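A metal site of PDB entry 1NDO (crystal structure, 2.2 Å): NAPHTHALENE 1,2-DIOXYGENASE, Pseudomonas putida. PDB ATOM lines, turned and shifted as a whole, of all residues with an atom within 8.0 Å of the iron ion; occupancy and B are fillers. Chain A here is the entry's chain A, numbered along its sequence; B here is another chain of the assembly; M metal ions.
ND2 of Asn 201 lies close to NE2 of His 208 (3.4 Å). The backbone carbonyl oxygen of His 208 sits close to the side-chain hydroxyl of Thr 212. The backbone carbonyl oxygen of Asp 205 sits at hydrogen-bond distance from a ring nitrogen (ND1) of His 208 (2.8 Å). A ring nitrogen (ND1) of His 213 lies within hydrogen-bond range of the side-chain carboxylate (OD2) of Asp 361 (2.8 Å). The side-chain hydroxyl (OH) of Tyr 103 of chain B lies within hydrogen-bond range of the side-chain amide nitrogen (ND2) of Asn 201 (3.0 Å).
Asn 201 touches the iron ion. Four residues have an atom within 4 Å of the iron ion: Asn 201, His 208, His 213 and Asp 362. The nearest printed residue that does not touch the iron ion is Thr 212 (4.5 Å).
The iron ion is bound by NE2 of His 208 (2.0 Å), NE2 of His 213 (2.2 Å) and OD2 of Asp 362 (2.3 Å). Slightly farther from the iron ion lies the side-chain carboxylate (OD1) of Asp 362 (2.7 Å).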
ATOM      1  N   ASN A 201       4.480 -18.727 -21.085  1.00  0.00           N
ATOM      2  CA  ASN A 201       3.189 -19.340 -20.906  1.00  0.00           C
ATOM      3  C   ASN A 201       3.331 -20.869 -20.979  1.00  0.00           C
ATOM      4  O   ASN A 201       2.834 -21.550 -20.106  1.00  0.00           O
ATOM      5  CB  ASN A 201       2.204 -18.813 -21.928  1.00  0.00           C
ATOM      6  CG  ASN A 201       0.856 -19.505 -21.759  1.00  0.00           C
ATOM      7  OD1 ASN A 201       0.601 -20.547 -22.371  1.00  0.00           O
ATOM      8  ND2 ASN A 201      -0.024 -18.975 -20.929  1.00  0.00           N
ATOM      9  N   PHE A 202       4.088 -21.383 -21.941  1.00  0.00           N
ATOM     10  CA  PHE A 202       4.267 -22.826 -22.087  1.00  0.00           C
ATOM     11  C   PHE A 202       5.253 -23.386 -21.079  1.00  0.00           C
ATOM     12  O   PHE A 202       5.165 -24.540 -20.668  1.00  0.00           O
ATOM     13  CB  PHE A 202       4.754 -23.078 -23.520  1.00  0.00           C
ATOM     14  CG  PHE A 202       3.668 -23.323 -24.524  1.00  0.00           C
ATOM     15  CD1 PHE A 202       2.761 -22.327 -24.833  1.00  0.00           C
ATOM     16  CD2 PHE A 202       3.532 -24.575 -25.116  1.00  0.00           C
ATOM     17  CE1 PHE A 202       1.753 -22.546 -25.730  1.00  0.00           C
ATOM     18  CE2 PHE A 202       2.524 -24.816 -26.055  1.00  0.00           C
ATOM     19  CZ  PHE A 202       1.641 -23.775 -26.334  1.00  0.00           C
ATOM     20  N   ASP A 205       3.138 -22.281 -17.112  1.00  0.00           N
ATOM     21  CA  ASP A 205       1.836 -21.751 -16.687  1.00  0.00           C
ATOM     22  C   ASP A 205       0.682 -22.739 -16.720  1.00  0.00           C
ATOM     23  O   ASP A 205      -0.100 -22.685 -17.670  1.00  0.00           O
ATOM     24  CB  ASP A 205       1.507 -20.502 -17.528  1.00  0.00           C
ATOM     25  CG  ASP A 205       0.345 -19.725 -16.938  1.00  0.00           C
ATOM     26  OD1 ASP A 205      -0.462 -20.211 -16.108  1.00  0.00           O
ATOM     27  OD2 ASP A 205       0.252 -18.571 -17.357  1.00  0.00           O
ATOM     28  N   ALA A 206       0.498 -23.466 -15.622  1.00  0.00           N
ATOM     29  CA  ALA A 206      -0.654 -24.372 -15.534  1.00  0.00           C
ATOM     30  C   ALA A 206      -1.803 -23.568 -14.922  1.00  0.00           C
ATOM     31  O   ALA A 206      -2.966 -23.761 -15.222  1.00  0.00           O
ATOM     32  CB  ALA A 206      -0.431 -25.632 -14.729  1.00  0.00           C
ATOM     33  N   HIS A 208      -3.194 -20.714 -15.666  1.00  0.00           N
ATOM     34  CA  HIS A 208      -4.144 -20.058 -16.526  1.00  0.00           C
ATOM     35  C   HIS A 208      -5.199 -20.967 -17.156  1.00  0.00           C
ATOM     36  O   HIS A 208      -6.187 -20.380 -17.643  1.00  0.00           O
ATOM     37  CB  HIS A 208      -3.391 -19.265 -17.639  1.00  0.00           C
ATOM     38  CG  HIS A 208      -2.984 -20.057 -18.818  1.00  0.00           C
ATOM     39  ND1 HIS A 208      -2.040 -21.051 -18.758  1.00  0.00           N
ATOM     40  CD2 HIS A 208      -3.409 -20.030 -20.099  1.00  0.00           C
ATOM     41  CE1 HIS A 208      -1.872 -21.608 -19.977  1.00  0.00           C
ATOM     42  NE2 HIS A 208      -2.710 -20.993 -20.791  1.00  0.00           N
ATOM     43  N   VAL A 209      -4.923 -22.243 -17.246  1.00  0.00           N
ATOM     44  CA  VAL A 209      -5.706 -23.182 -18.011  1.00  0.00           C
ATOM     45  C   VAL A 209      -7.197 -23.160 -17.751  1.00  0.00           C
ATOM     46  O   VAL A 209      -8.002 -22.940 -18.697  1.00  0.00           O
ATOM     47  CB  VAL A 209      -5.178 -24.636 -17.919  1.00  0.00           C
ATOM     48  CG1 VAL A 209      -6.051 -25.552 -18.771  1.00  0.00           C
ATOM     49  CG2 VAL A 209      -3.719 -24.685 -18.418  1.00  0.00           C
ATOM     50  N   GLY A 210      -7.633 -23.374 -16.533  1.00  0.00           N
ATOM     51  CA  GLY A 210      -9.021 -23.476 -16.174  1.00  0.00           C
ATOM     52  C   GLY A 210      -9.826 -22.214 -16.460  1.00  0.00           C
ATOM     53  O   GLY A 210     -11.024 -22.236 -16.818  1.00  0.00           O
ATOM     54  N   THR A 212      -8.474 -19.159 -18.562  1.00  0.00           N
ATOM     55  CA  THR A 212      -8.289 -18.808 -19.956  1.00  0.00           C
ATOM     56  C   THR A 212      -8.962 -19.831 -20.889  1.00  0.00           C
ATOM     57  O   THR A 212      -9.603 -19.391 -21.844  1.00  0.00           O
ATOM     58  CB  THR A 212      -6.795 -18.742 -20.354  1.00  0.00           C
ATOM     59  OG1 THR A 212      -6.162 -17.611 -19.777  1.00  0.00           O
ATOM     60  CG2 THR A 212      -6.573 -18.716 -21.884  1.00  0.00           C
ATOM     61  N   HIS A 213      -8.801 -21.133 -20.652  1.00  0.00           N
ATOM     62  CA  HIS A 213      -9.311 -22.134 -21.567  1.00  0.00           C
ATOM     63  C   HIS A 213     -10.671 -22.709 -21.166  1.00  0.00           C
ATOM     64  O   HIS A 213     -11.096 -23.708 -21.746  1.00  0.00           O
ATOM     65  CB  HIS A 213      -8.257 -23.267 -21.729  1.00  0.00           C
ATOM     66  CG  HIS A 213      -7.051 -22.735 -22.427  1.00  0.00           C
ATOM     67  ND1 HIS A 213      -7.124 -22.222 -23.696  1.00  0.00           N
ATOM     68  CD2 HIS A 213      -5.761 -22.600 -22.045  1.00  0.00           C
ATOM     69  CE1 HIS A 213      -5.932 -21.794 -24.112  1.00  0.00           C
ATOM     70  NE2 HIS A 213      -5.102 -22.021 -23.105  1.00  0.00           N
ATOM     71  N   LEU A 307       4.215 -29.479 -25.969  1.00  0.00           N
ATOM     72  CA  LEU A 307       3.380 -30.246 -25.028  1.00  0.00           C
ATOM     73  C   LEU A 307       3.591 -31.707 -25.355  1.00  0.00           C
ATOM     74  O   LEU A 307       3.055 -32.125 -26.408  1.00  0.00           O
ATOM     75  CB  LEU A 307       1.900 -29.849 -25.099  1.00  0.00           C
ATOM     76  CG  LEU A 307       1.480 -28.368 -25.063  1.00  0.00           C
ATOM     77  CD1 LEU A 307      -0.062 -28.273 -25.129  1.00  0.00           C
ATOM     78  CD2 LEU A 307       1.937 -27.707 -23.790  1.00  0.00           C
ATOM     79  N   PHE A 352      -4.278 -26.296 -31.353  1.00  0.00           N
ATOM     80  CA  PHE A 352      -3.198 -25.339 -31.190  1.00  0.00           C
ATOM     81  C   PHE A 352      -2.610 -24.739 -32.456  1.00  0.00           C
ATOM     82  O   PHE A 352      -1.588 -24.040 -32.411  1.00  0.00           O
ATOM     83  CB  PHE A 352      -2.073 -26.005 -30.370  1.00  0.00           C
ATOM     84  CG  PHE A 352      -2.331 -25.914 -28.899  1.00  0.00           C
ATOM     85  CD1 PHE A 352      -1.929 -24.831 -28.153  1.00  0.00           C
ATOM     86  CD2 PHE A 352      -3.022 -26.929 -28.236  1.00  0.00           C
ATOM     87  CE1 PHE A 352      -2.158 -24.727 -26.786  1.00  0.00           C
ATOM     88  CE2 PHE A 352      -3.269 -26.849 -26.878  1.00  0.00           C
ATOM     89  CZ  PHE A 352      -2.848 -25.764 -26.165  1.00  0.00           C
ATOM     90  N   TRP A 358      -7.927 -23.775 -28.700  1.00  0.00           N
ATOM     91  CA  TRP A 358      -7.239 -23.408 -27.445  1.00  0.00           C
ATOM     92  C   TRP A 358      -6.262 -22.267 -27.680  1.00  0.00           C
ATOM     93  O   TRP A 358      -6.203 -21.277 -26.979  1.00  0.00           O
ATOM     94  CB  TRP A 358      -6.476 -24.538 -26.799  1.00  0.00           C
ATOM     95  CG  TRP A 358      -7.219 -25.782 -26.404  1.00  0.00           C
ATOM     96  CD1 TRP A 358      -8.069 -26.576 -27.131  1.00  0.00           C
ATOM     97  CD2 TRP A 358      -7.139 -26.359 -25.096  1.00  0.00           C
ATOM     98  NE1 TRP A 358      -8.519 -27.629 -26.358  1.00  0.00           N
ATOM     99  CE2 TRP A 358      -7.939 -27.525 -25.112  1.00  0.00           C
ATOM    100  CE3 TRP A 358      -6.425 -26.012 -23.936  1.00  0.00           C
ATOM    101  CZ2 TRP A 358      -8.068 -28.330 -23.982  1.00  0.00           C
ATOM    102  CZ3 TRP A 358      -6.566 -26.827 -22.832  1.00  0.00           C
ATOM    103  CH2 TRP A 358      -7.383 -27.963 -22.856  1.00  0.00           C
ATOM    104  N   GLU A 359      -5.338 -22.340 -28.603  1.00  0.00           N
ATOM    105  CA  GLU A 359      -4.353 -21.324 -28.934  1.00  0.00           C
ATOM    106  C   GLU A 359      -5.038 -19.952 -29.112  1.00  0.00           C
ATOM    107  O   GLU A 359      -4.627 -18.951 -28.530  1.00  0.00           O
ATOM    108  CB  GLU A 359      -3.590 -21.735 -30.188  1.00  0.00           C
ATOM    109  CG  GLU A 359      -2.598 -20.729 -30.762  1.00  0.00           C
ATOM    110  CD  GLU A 359      -1.195 -20.937 -30.244  1.00  0.00           C
ATOM    111  OE1 GLU A 359      -1.040 -21.556 -29.171  1.00  0.00           O
ATOM    112  OE2 GLU A 359      -0.253 -20.449 -30.933  1.00  0.00           O
ATOM    113  N   SER A 360      -6.173 -19.876 -29.776  1.00  0.00           N
ATOM    114  CA  SER A 360      -6.932 -18.658 -29.941  1.00  0.00           C
ATOM    115  C   SER A 360      -7.378 -18.045 -28.630  1.00  0.00           C
ATOM    116  O   SER A 360      -7.436 -16.817 -28.510  1.00  0.00           O
ATOM    117  CB  SER A 360      -8.147 -18.939 -30.871  1.00  0.00           C
ATOM    118  OG  SER A 360      -7.526 -19.291 -32.143  1.00  0.00           O
ATOM    119  N   ASP A 361      -7.667 -18.817 -27.581  1.00  0.00           N
ATOM    120  CA  ASP A 361      -8.036 -18.293 -26.297  1.00  0.00           C
ATOM    121  C   ASP A 361      -6.840 -17.514 -25.701  1.00  0.00           C
ATOM    122  O   ASP A 361      -7.029 -16.757 -24.768  1.00  0.00           O
ATOM    123  CB  ASP A 361      -8.350 -19.416 -25.307  1.00  0.00           C
ATOM    124  CG  ASP A 361      -9.476 -20.371 -25.586  1.00  0.00           C
ATOM    125  OD1 ASP A 361     -10.498 -20.044 -26.235  1.00  0.00           O
ATOM    126  OD2 ASP A 361      -9.366 -21.526 -25.136  1.00  0.00           O
ATOM    127  N   ASP A 362      -5.579 -17.833 -26.071  1.00  0.00           N
ATOM    128  CA  ASP A 362      -4.416 -17.203 -25.493  1.00  0.00           C
ATOM    129  C   ASP A 362      -4.029 -15.880 -26.174  1.00  0.00           C
ATOM    130  O   ASP A 362      -3.161 -15.203 -25.605  1.00  0.00           O
ATOM    131  CB  ASP A 362      -3.229 -18.165 -25.608  1.00  0.00           C
ATOM    132  CG  ASP A 362      -3.176 -19.197 -24.521  1.00  0.00           C
ATOM    133  OD1 ASP A 362      -3.384 -18.828 -23.336  1.00  0.00           O
ATOM    134  OD2 ASP A 362      -2.909 -20.392 -24.782  1.00  0.00           O
ATOM    135  N   ASN A 363      -4.505 -15.581 -27.374  1.00  0.00           N
ATOM    136  CA  ASN A 363      -4.064 -14.451 -28.158  1.00  0.00           C
ATOM    137  C   ASN A 363      -4.128 -13.135 -27.417  1.00  0.00           C
ATOM    138  O   ASN A 363      -3.158 -12.393 -27.472  1.00  0.00           O
ATOM    139  CB  ASN A 363      -4.939 -14.200 -29.393  1.00  0.00           C
ATOM    140  CG  ASN A 363      -4.646 -15.000 -30.628  1.00  0.00           C
ATOM    141  OD1 ASN A 363      -5.329 -14.794 -31.636  1.00  0.00           O
ATOM    142  ND2 ASN A 363      -3.676 -15.905 -30.607  1.00  0.00           N
ATOM    143  N   ASN A 365      -4.307 -12.609 -24.284  1.00  0.00           N
ATOM    144  CA  ASN A 365      -3.436 -12.620 -23.123  1.00  0.00           C
ATOM    145  C   ASN A 365      -2.018 -12.143 -23.501  1.00  0.00           C
ATOM    146  O   ASN A 365      -1.409 -11.278 -22.871  1.00  0.00           O
ATOM    147  CB  ASN A 365      -3.378 -14.025 -22.548  1.00  0.00           C
ATOM    148  CG  ASN A 365      -4.662 -14.453 -21.860  1.00  0.00           C
ATOM    149  OD1 ASN A 365      -5.513 -13.625 -21.524  1.00  0.00           O
ATOM    150  ND2 ASN A 365      -4.780 -15.757 -21.618  1.00  0.00           N
ATOM    151  N   MET A 366      -1.475 -12.795 -24.516  1.00  0.00           N
ATOM    152  CA  MET A 366      -0.153 -12.632 -25.011  1.00  0.00           C
ATOM    153  C   MET A 366       0.024 -11.217 -25.629  1.00  0.00           C
ATOM    154  O   MET A 366       1.057 -10.593 -25.388  1.00  0.00           O
ATOM    155  CB  MET A 366       0.241 -13.573 -26.143  1.00  0.00           C
ATOM    156  CG  MET A 366      -0.103 -15.045 -26.120  1.00  0.00           C
ATOM    157  SD  MET A 366       1.069 -15.855 -25.068  1.00  0.00           S
ATOM    158  CE  MET A 366       0.559 -15.402 -23.432  1.00  0.00           C
ATOM    159  N   TYR B 103      -6.793 -13.706 -17.921  1.00  0.00           N
ATOM    160  CA  TYR B 103      -5.613 -14.524 -18.041  1.00  0.00           C
ATOM    161  C   TYR B 103      -5.648 -15.555 -16.898  1.00  0.00           C
ATOM    162  O   TYR B 103      -5.862 -16.727 -17.196  1.00  0.00           O
ATOM    163  CB  TYR B 103      -4.303 -13.735 -18.071  1.00  0.00           C
ATOM    164  CG  TYR B 103      -3.063 -14.357 -18.641  1.00  0.00           C
ATOM    165  CD1 TYR B 103      -2.989 -15.727 -18.896  1.00  0.00           C
ATOM    166  CD2 TYR B 103      -1.929 -13.591 -18.927  1.00  0.00           C
ATOM    167  CE1 TYR B 103      -1.842 -16.318 -19.420  1.00  0.00           C
ATOM    168  CE2 TYR B 103      -0.771 -14.127 -19.439  1.00  0.00           C
ATOM    169  CZ  TYR B 103      -0.739 -15.494 -19.681  1.00  0.00           C
ATOM    170  OH  TYR B 103       0.389 -16.084 -20.182  1.00  0.00           O
HETATM  171 FE    FE M   1      -3.075 -21.398 -22.750  1.00  0.00          FE
